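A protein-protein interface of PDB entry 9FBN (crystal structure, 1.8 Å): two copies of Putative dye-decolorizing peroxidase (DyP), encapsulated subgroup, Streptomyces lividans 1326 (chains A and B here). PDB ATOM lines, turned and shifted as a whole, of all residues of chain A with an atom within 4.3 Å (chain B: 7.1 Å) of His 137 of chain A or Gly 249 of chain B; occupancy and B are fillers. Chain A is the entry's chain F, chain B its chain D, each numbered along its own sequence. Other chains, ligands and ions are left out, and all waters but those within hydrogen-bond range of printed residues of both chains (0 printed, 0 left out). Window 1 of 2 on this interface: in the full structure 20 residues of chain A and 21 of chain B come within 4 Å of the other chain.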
ATOM      1  N   ALA A  21      -6.455   3.306 -17.179  1.00  0.00           N
ATOM      2  CA  ALA A  21      -7.464   4.357 -17.001  1.00  0.00           C
ATOM      3  C   ALA A  21      -7.897   4.915 -18.353  1.00  0.00           C
ATOM      4  O   ALA A  21      -7.114   4.899 -19.275  1.00  0.00           O
ATOM      5  CB  ALA A  21      -6.892   5.529 -16.155  1.00  0.00           C
ATOM      6  N   ILE A  22      -9.111   5.525 -18.394  1.00  0.00           N
ATOM      7  CA  ILE A  22      -9.525   6.495 -19.401  1.00  0.00           C
ATOM      8  C   ILE A  22      -9.917   7.792 -18.682  1.00  0.00           C
ATOM      9  O   ILE A  22     -10.655   7.799 -17.675  1.00  0.00           O
ATOM     10  CB  ILE A  22     -10.688   5.908 -20.236  1.00  0.00           C
ATOM     11  CG1 ILE A  22     -10.161   4.725 -21.058  1.00  0.00           C
ATOM     12  CG2 ILE A  22     -11.355   6.975 -21.103  1.00  0.00           C
ATOM     13  CD1 ILE A  22     -11.178   4.051 -21.945  1.00  0.00           C
ATOM     14  N   PHE A 116     -13.108   1.029 -21.156  1.00  0.00           N
ATOM     15  CA  PHE A 116     -13.719   1.389 -22.440  1.00  0.00           C
ATOM     16  C   PHE A 116     -15.214   1.079 -22.465  1.00  0.00           C
ATOM     17  O   PHE A 116     -15.953   1.876 -22.987  1.00  0.00           O
ATOM     18  CB  PHE A 116     -12.977   0.695 -23.571  1.00  0.00           C
ATOM     19  CG  PHE A 116     -13.309   1.212 -24.963  1.00  0.00           C
ATOM     20  CD1 PHE A 116     -12.598   2.255 -25.512  1.00  0.00           C
ATOM     21  CD2 PHE A 116     -14.341   0.673 -25.717  1.00  0.00           C
ATOM     22  CE1 PHE A 116     -12.878   2.744 -26.789  1.00  0.00           C
ATOM     23  CE2 PHE A 116     -14.628   1.178 -26.979  1.00  0.00           C
ATOM     24  CZ  PHE A 116     -13.901   2.181 -27.524  1.00  0.00           C
ATOM     25  N   GLU A 135      -9.708  12.878 -24.469  1.00  0.00           N
ATOM     26  CA  GLU A 135      -9.850  11.480 -24.281  1.00  0.00           C
ATOM     27  C   GLU A 135      -8.398  10.933 -24.273  1.00  0.00           C
ATOM     28  O   GLU A 135      -7.640  11.123 -25.230  1.00  0.00           O
ATOM     29  CB  GLU A 135     -10.634  10.758 -25.370  1.00  0.00           C
ATOM     30  CG  GLU A 135     -10.699   9.254 -25.188  1.00  0.00           C
ATOM     31  CD  GLU A 135     -11.610   8.582 -26.193  1.00  0.00           C
ATOM     32  OE1 GLU A 135     -12.200   9.327 -27.017  1.00  0.00           O
ATOM     33  OE2 GLU A 135     -11.920   7.384 -26.000  1.00  0.00           O
ATOM     34  N   VAL A 136      -8.038  10.321 -23.145  1.00  0.00           N
ATOM     35  CA  VAL A 136      -6.691   9.755 -22.946  1.00  0.00           C
ATOM     36  C   VAL A 136      -6.860   8.365 -22.387  1.00  0.00           C
ATOM     37  O   VAL A 136      -7.547   8.115 -21.367  1.00  0.00           O
ATOM     38  CB  VAL A 136      -5.738  10.617 -22.096  1.00  0.00           C
ATOM     39  CG1 VAL A 136      -4.428   9.895 -21.737  1.00  0.00           C
ATOM     40  CG2 VAL A 136      -5.386  11.960 -22.743  1.00  0.00           C
ATOM     41  N   HIS A 137      -6.184   7.436 -23.071  1.00  0.00           N
ATOM     42  CA  HIS A 137      -6.057   6.079 -22.631  1.00  0.00           C
ATOM     43  C   HIS A 137      -4.725   5.939 -21.882  1.00  0.00           C
ATOM     44  O   HIS A 137      -3.716   5.883 -22.531  1.00  0.00           O
ATOM     45  CB  HIS A 137      -6.255   5.129 -23.830  1.00  0.00           C
ATOM     46  CG  HIS A 137      -7.588   5.297 -24.558  1.00  0.00           C
ATOM     47  ND1 HIS A 137      -7.898   4.499 -25.639  1.00  0.00           N
ATOM     48  CD2 HIS A 137      -8.686   6.061 -24.356  1.00  0.00           C
ATOM     49  CE1 HIS A 137      -9.154   4.786 -26.077  1.00  0.00           C
ATOM     50  NE2 HIS A 137      -9.662   5.738 -25.307  1.00  0.00           N
ATOM     51  N   GLY A 138      -4.755   5.651 -20.560  1.00  0.00           N
ATOM     52  CA  GLY A 138      -3.456   5.515 -19.872  1.00  0.00           C
ATOM     53  C   GLY A 138      -3.133   4.096 -19.450  1.00  0.00           C
ATOM     54  O   GLY A 138      -4.010   3.243 -19.356  1.00  0.00           O
ATOM     55  N   PHE A 139      -1.822   3.827 -19.211  1.00  0.00           N
ATOM     56  CA  PHE A 139      -1.312   2.531 -18.896  1.00  0.00           C
ATOM     57  C   PHE A 139      -0.076   2.715 -17.983  1.00  0.00           C
ATOM     58  O   PHE A 139       0.796   3.503 -18.256  1.00  0.00           O
ATOM     59  CB  PHE A 139      -0.911   1.687 -20.101  1.00  0.00           C
ATOM     60  CG  PHE A 139      -0.021   2.405 -21.089  1.00  0.00           C
ATOM     61  CD1 PHE A 139       1.365   2.291 -20.995  1.00  0.00           C
ATOM     62  CD2 PHE A 139      -0.576   3.134 -22.123  1.00  0.00           C
ATOM     63  CE1 PHE A 139       2.167   2.979 -21.907  1.00  0.00           C
ATOM     64  CE2 PHE A 139       0.234   3.782 -23.039  1.00  0.00           C
ATOM     65  CZ  PHE A 139       1.608   3.696 -22.910  1.00  0.00           C
ATOM     66  N   PHE A 248       0.819   7.863 -21.171  1.00  0.00           N
ATOM     67  CA  PHE A 248       0.064   7.650 -22.387  1.00  0.00           C
ATOM     68  C   PHE A 248       0.932   8.124 -23.535  1.00  0.00           C
ATOM     69  O   PHE A 248       1.952   8.788 -23.287  1.00  0.00           O
ATOM     70  CB  PHE A 248      -1.250   8.458 -22.410  1.00  0.00           C
ATOM     71  CG  PHE A 248      -1.048   9.952 -22.513  1.00  0.00           C
ATOM     72  CD1 PHE A 248      -0.762  10.710 -21.399  1.00  0.00           C
ATOM     73  CD2 PHE A 248      -0.875  10.528 -23.783  1.00  0.00           C
ATOM     74  CE1 PHE A 248      -0.505  12.054 -21.492  1.00  0.00           C
ATOM     75  CE2 PHE A 248      -0.567  11.852 -23.908  1.00  0.00           C
ATOM     76  CZ  PHE A 248      -0.394  12.629 -22.758  1.00  0.00           C
ATOM     77  N   LEU B 112      -0.400  -3.534 -21.966  1.00  0.00           N
ATOM     78  CA  LEU B 112      -0.071  -2.566 -23.019  1.00  0.00           C
ATOM     79  C   LEU B 112       1.287  -1.886 -22.831  1.00  0.00           C
ATOM     80  O   LEU B 112       1.861  -1.472 -23.831  1.00  0.00           O
ATOM     81  CB  LEU B 112      -1.163  -1.527 -23.168  1.00  0.00           C
ATOM     82  CG  LEU B 112      -1.171  -0.673 -24.442  1.00  0.00           C
ATOM     83  CD1 LEU B 112      -1.059  -1.559 -25.693  1.00  0.00           C
ATOM     84  CD2 LEU B 112      -2.442   0.165 -24.536  1.00  0.00           C
ATOM     85  N   VAL B 136      -2.107   0.968 -34.143  1.00  0.00           N
ATOM     86  CA  VAL B 136      -3.330   0.549 -33.503  1.00  0.00           C
ATOM     87  C   VAL B 136      -2.979  -0.114 -32.166  1.00  0.00           C
ATOM     88  O   VAL B 136      -2.103  -0.986 -32.135  1.00  0.00           O
ATOM     89  CB  VAL B 136      -4.168  -0.402 -34.395  1.00  0.00           C
ATOM     90  CG1 VAL B 136      -5.210  -1.100 -33.555  1.00  0.00           C
ATOM     91  CG2 VAL B 136      -4.728   0.309 -35.635  1.00  0.00           C
ATOM     92  N   HIS B 137      -3.591   0.389 -31.065  1.00  0.00           N
ATOM     93  CA  HIS B 137      -3.437  -0.252 -29.757  1.00  0.00           C
ATOM     94  C   HIS B 137      -4.683  -1.099 -29.479  1.00  0.00           C
ATOM     95  O   HIS B 137      -5.754  -0.515 -29.353  1.00  0.00           O
ATOM     96  CB  HIS B 137      -3.218   0.845 -28.673  1.00  0.00           C
ATOM     97  CG  HIS B 137      -2.049   1.782 -28.920  1.00  0.00           C
ATOM     98  ND1 HIS B 137      -1.709   2.837 -28.084  1.00  0.00           N
ATOM     99  CD2 HIS B 137      -1.095   1.791 -29.878  1.00  0.00           C
ATOM    100  CE1 HIS B 137      -0.608   3.434 -28.547  1.00  0.00           C
ATOM    101  NE2 HIS B 137      -0.233   2.817 -29.622  1.00  0.00           N
ATOM    102  N   GLY B 138      -4.554  -2.422 -29.369  1.00  0.00           N
ATOM    103  CA  GLY B 138      -5.725  -3.260 -29.251  1.00  0.00           C
ATOM    104  C   GLY B 138      -5.858  -3.761 -27.817  1.00  0.00           C
ATOM    105  O   GLY B 138      -4.850  -3.838 -27.144  1.00  0.00           O
ATOM    106  N   PHE B 139      -7.087  -4.139 -27.478  1.00  0.00           N
ATOM    107  CA  PHE B 139      -7.411  -4.727 -26.190  1.00  0.00           C
ATOM    108  C   PHE B 139      -8.513  -5.755 -26.417  1.00  0.00           C
ATOM    109  O   PHE B 139      -9.573  -5.436 -26.954  1.00  0.00           O
ATOM    110  CB  PHE B 139      -7.712  -3.599 -25.181  1.00  0.00           C
ATOM    111  CG  PHE B 139      -8.752  -2.613 -25.664  1.00  0.00           C
ATOM    112  CD1 PHE B 139     -10.100  -2.911 -25.552  1.00  0.00           C
ATOM    113  CD2 PHE B 139      -8.414  -1.457 -26.327  1.00  0.00           C
ATOM    114  CE1 PHE B 139     -11.040  -2.048 -26.028  1.00  0.00           C
ATOM    115  CE2 PHE B 139      -9.375  -0.576 -26.738  1.00  0.00           C
ATOM    116  CZ  PHE B 139     -10.687  -0.879 -26.603  1.00  0.00           C
ATOM    117  N   MET B 147     -15.908  -6.357 -30.571  1.00  0.00           N
ATOM    118  CA  MET B 147     -16.712  -5.155 -30.611  1.00  0.00           C
ATOM    119  C   MET B 147     -18.152  -5.490 -31.015  1.00  0.00           C
ATOM    120  O   MET B 147     -19.063  -4.789 -30.580  1.00  0.00           O
ATOM    121  CB  MET B 147     -15.986  -4.191 -31.564  1.00  0.00           C
ATOM    122  CG  MET B 147     -16.291  -2.762 -31.401  1.00  0.00           C
ATOM    123  SD  MET B 147     -15.979  -2.044 -29.771  1.00  0.00           S
ATOM    124  CE  MET B 147     -14.227  -1.838 -30.066  1.00  0.00           C
ATOM    125  N   LEU B 187     -13.879  -0.721 -39.264  1.00  0.00           N
ATOM    126  CA  LEU B 187     -14.680   0.169 -38.451  1.00  0.00           C
ATOM    127  C   LEU B 187     -16.147  -0.266 -38.548  1.00  0.00           C
ATOM    128  O   LEU B 187     -16.566  -0.661 -39.653  1.00  0.00           O
ATOM    129  CB  LEU B 187     -14.503   1.615 -38.940  1.00  0.00           C
ATOM    130  CG  LEU B 187     -13.094   2.187 -38.817  1.00  0.00           C
ATOM    131  CD1 LEU B 187     -12.959   3.557 -39.450  1.00  0.00           C
ATOM    132  CD2 LEU B 187     -12.721   2.237 -37.364  1.00  0.00           C
ATOM    133  N   PRO B 247      -9.979  -5.834 -30.755  1.00  0.00           N
ATOM    134  CA  PRO B 247     -10.836  -4.648 -30.668  1.00  0.00           C
ATOM    135  C   PRO B 247      -9.935  -3.421 -30.487  1.00  0.00           C
ATOM    136  O   PRO B 247      -8.841  -3.538 -29.936  1.00  0.00           O
ATOM    137  CB  PRO B 247     -11.681  -4.915 -29.356  1.00  0.00           C
ATOM    138  CG  PRO B 247     -11.694  -6.404 -29.318  1.00  0.00           C
ATOM    139  CD  PRO B 247     -10.218  -6.679 -29.564  1.00  0.00           C
ATOM    140  N   PHE B 248     -10.372  -2.290 -30.960  1.00  0.00           N
ATOM    141  CA  PHE B 248      -9.732  -0.969 -30.742  1.00  0.00           C
ATOM    142  C   PHE B 248     -10.785   0.108 -30.895  1.00  0.00           C
ATOM    143  O   PHE B 248     -11.861  -0.108 -31.494  1.00  0.00           O
ATOM    144  CB  PHE B 248      -8.572  -0.752 -31.696  1.00  0.00           C
ATOM    145  CG  PHE B 248      -9.019  -0.451 -33.117  1.00  0.00           C
ATOM    146  CD1 PHE B 248      -9.277  -1.500 -34.019  1.00  0.00           C
ATOM    147  CD2 PHE B 248      -9.296   0.843 -33.547  1.00  0.00           C
ATOM    148  CE1 PHE B 248      -9.621  -1.198 -35.332  1.00  0.00           C
ATOM    149  CE2 PHE B 248      -9.656   1.142 -34.877  1.00  0.00           C
ATOM    150  CZ  PHE B 248      -9.913   0.107 -35.742  1.00  0.00           C
ATOM    151  N   GLY B 249     -10.493   1.338 -30.391  1.00  0.00           N
ATOM    152  CA  GLY B 249     -11.458   2.390 -30.650  1.00  0.00           C
ATOM    153  C   GLY B 249     -11.208   3.663 -29.824  1.00  0.00           C
ATOM    154  O   GLY B 249     -10.155   3.798 -29.202  1.00  0.00           O
ATOM    155  N   SER B 250     -12.169   4.583 -29.951  1.00  0.00           N
ATOM    156  CA  SER B 250     -12.118   5.897 -29.327  1.00  0.00           C
ATOM    157  C   SER B 250     -13.559   6.319 -29.083  1.00  0.00           C
ATOM    158  O   SER B 250     -14.321   6.446 -30.039  1.00  0.00           O
ATOM    159  CB  SER B 250     -11.344   6.912 -30.199  1.00  0.00           C
ATOM    160  OG  SER B 250     -11.682   8.235 -29.795  1.00  0.00           O
ATOM    161  N   VAL B 251     -13.930   6.545 -27.795  1.00  0.00           N
ATOM    162  CA  VAL B 251     -15.316   6.799 -27.490  1.00  0.00           C
ATOM    163  C   VAL B 251     -15.749   8.143 -28.055  1.00  0.00           C
ATOM    164  O   VAL B 251     -16.899   8.277 -28.479  1.00  0.00           O
ATOM    165  CB  VAL B 251     -15.648   6.630 -26.002  1.00  0.00           C
ATOM    166  CG1 VAL B 251     -17.111   6.961 -25.743  1.00  0.00           C
ATOM    167  CG2 VAL B 251     -15.364   5.204 -25.591  1.00  0.00           C
ATOM    168  N   GLY B 252     -14.864   9.143 -28.035  1.00  0.00           N
ATOM    169  CA  GLY B 252     -15.213  10.502 -28.400  1.00  0.00           C
ATOM    170  C   GLY B 252     -15.441  10.682 -29.909  1.00  0.00           C
ATOM    171  O   GLY B 252     -16.314  11.446 -30.311  1.00  0.00           O
ATOM    172  N   ARG B 253     -14.630  10.017 -30.729  1.00  0.00           N
ATOM    173  CA  ARG B 253     -14.784  10.077 -32.173  1.00  0.00           C
ATOM    174  C   ARG B 253     -15.691   8.955 -32.693  1.00  0.00           C
ATOM    175  O   ARG B 253     -15.777   8.783 -33.890  1.00  0.00           O
ATOM    176  CB  ARG B 253     -13.425   9.993 -32.869  1.00  0.00           C
ATOM    177  CG  ARG B 253     -12.449  11.047 -32.383  1.00  0.00           C
ATOM    178  CD  ARG B 253     -11.150  11.032 -33.174  1.00  0.00           C
ATOM    179  NE  ARG B 253     -10.533   9.701 -33.307  1.00  0.00           N
ATOM    180  CZ  ARG B 253      -9.413   9.268 -32.709  1.00  0.00           C
ATOM    181  NH1 ARG B 253      -8.746  10.073 -31.896  1.00  0.00           N
ATOM    182  NH2 ARG B 253      -8.975   8.025 -32.914  1.00  0.00           N
ATOM    183  N   GLU B 254     -16.428   8.215 -31.845  1.00  0.00           N
ATOM    184  CA  GLU B 254     -17.336   7.204 -32.367  1.00  0.00           C
ATOM    185  C   GLU B 254     -16.598   6.268 -33.323  1.00  0.00           C
ATOM    186  O   GLU B 254     -17.036   5.967 -34.437  1.00  0.00           O
ATOM    187  CB  GLU B 254     -18.549   7.892 -32.988  1.00  0.00           C
ATOM    188  CG  GLU B 254     -19.234   8.874 -32.044  1.00  0.00           C
ATOM    189  CD  GLU B 254     -20.374   9.606 -32.741  1.00  0.00           C
ATOM    190  OE1 GLU B 254     -21.326   8.894 -33.169  1.00  0.00           O
ATOM    191  OE2 GLU B 254     -20.293  10.860 -32.869  1.00  0.00           O
ATOM    192  N   GLU B 255     -15.465   5.752 -32.850  1.00  0.00           N
ATOM    193  CA  GLU B 255     -14.652   4.842 -33.638  1.00  0.00           C
ATOM    194  C   GLU B 255     -14.611   3.556 -32.844  1.00  0.00           C
ATOM    195  O   GLU B 255     -14.141   3.565 -31.707  1.00  0.00           O
ATOM    196  CB  GLU B 255     -13.332   5.554 -33.929  1.00  0.00           C
ATOM    197  CG  GLU B 255     -12.133   4.678 -34.234  1.00  0.00           C
ATOM    198  CD  GLU B 255     -10.949   5.494 -34.734  1.00  0.00           C
ATOM    199  OE1 GLU B 255     -11.157   6.671 -35.195  1.00  0.00           O
ATOM    200  OE2 GLU B 255      -9.820   4.935 -34.680  1.00  0.00           O
ATOM    201  N   PHE B 256     -15.221   2.497 -33.399  1.00  0.00           N
ATOM    202  CA  PHE B 256     -15.334   1.198 -32.792  1.00  0.00           C
ATOM    203  C   PHE B 256     -14.943   0.157 -33.834  1.00  0.00           C
ATOM    204  O   PHE B 256     -15.599   0.066 -34.837  1.00  0.00           O
ATOM    205  CB  PHE B 256     -16.722   0.915 -32.259  1.00  0.00           C
ATOM    206  CG  PHE B 256     -17.250   1.967 -31.300  1.00  0.00           C
ATOM    207  CD1 PHE B 256     -16.987   1.860 -29.944  1.00  0.00           C
ATOM    208  CD2 PHE B 256     -18.064   2.990 -31.746  1.00  0.00           C
ATOM    209  CE1 PHE B 256     -17.473   2.811 -29.060  1.00  0.00           C
ATOM    210  CE2 PHE B 256     -18.571   3.912 -30.841  1.00  0.00           C
ATOM    211  CZ  PHE B 256     -18.259   3.809 -29.507  1.00  0.00           C
ATOM    212  N   GLY B 257     -13.820  -0.527 -33.622  1.00  0.00           N
ATOM    213  CA  GLY B 257     -13.207  -1.270 -34.709  1.00  0.00           C
ATOM    214  C   GLY B 257     -12.743  -2.649 -34.273  1.00  0.00           C
ATOM    215  O   GLY B 257     -12.839  -3.065 -33.082  1.00  0.00           O
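The side-chain carboxylate of Glu 135 of chain A is in hydrogen-bond range of a ring nitrogen (NE2) of His 137 of chain A (2.9 Å). The backbone NH (N) of Ser 250 of chain B is in hydrogen-bond range of the backbone carbonyl oxygen (O) of Glu 255 of chain B, at 2.8 Å. The backbone NH (N) of Phe 139 of chain B sits at hydrogen-bond distance from the backbone carbonyl oxygen (O) of Pro 247 of chain B (3.1 Å).
Phe 116 of chain A touches Phe 139 of chain B (CG to CZ, 3.7 Å). CE1 of Phe 116 of chain A touches C of Gly 249 of chain B, 3.6 Å away. CE1 of Phe 116 of chain A touches N of Ser 250 of chain B, at 3.7 Å. Phe 116 of chain A touches Val 251 of chain B. Phe 116 of chain A touches Phe 256 of chain B (CE2 to CD1, 3.8 Å). His 137 of chain A touches Gly 249 of chain B (CE1 to O, 3.4 Å).
N of Gly 252 of chain B lies within hydrogen-bond range of OE1 of Glu 135 of chain A. OG of Ser 250 of chain B lies within hydrogen-bond range of OE1 of Glu 135 of chain A, 3.0 Å away. The backbone NH (N) of Val 251 of chain B lies within hydrogen-bond range of the side-chain carboxylate (OE2) of Glu 135 of chain A (2.8 Å).
Hydrophobic or aromatic side chains of chain A within 4 Å of the printed part of chain B: Phe 116 and His 137. Of the 18 printed residues of chain B, 6 touch a printed residue of chain A. Hydrophobic or aromatic side chains of chain B that line the printed part of chain A: Phe 139, Val 251 and Phe 256. Among the printed residues, 9 pairs touch across the chains.
5 positions are printed for both chains. Of the 9 pairs that touch across the chains among the printed residues, none has its exchanged pair printed and touching as well.
Of the printed residues of chain B, Glu 135 of chain A touches Ser 250 (3.0 Å), Val 251 (2.8 Å) and Gly 252 (2.9 Å). His 137 of chain A touches just one residue of chain B: Gly 249 (3.4 Å). Phe 248 of chain A touches none of the printed residues of chain B. Of chain A, only Phe 116 (3.6 Å) and His 137 (3.4 Å) come within 4 Å of Gly 249 of chain B. Printed residues of chain A within 4 Å of Ser 250 of chain B: Phe 116 and Glu 135. Printed residues of chain A within 4 Å of Val 251 of chain B: Phe 116 (3.7 Å) and Glu 135 (2.8 Å). Arg 253 of chain B touches none of the printed residues of chain A. The nearest residue of chain B that does not touch His 137 of chain A is Ser 250 of chain B (4.5 Å).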
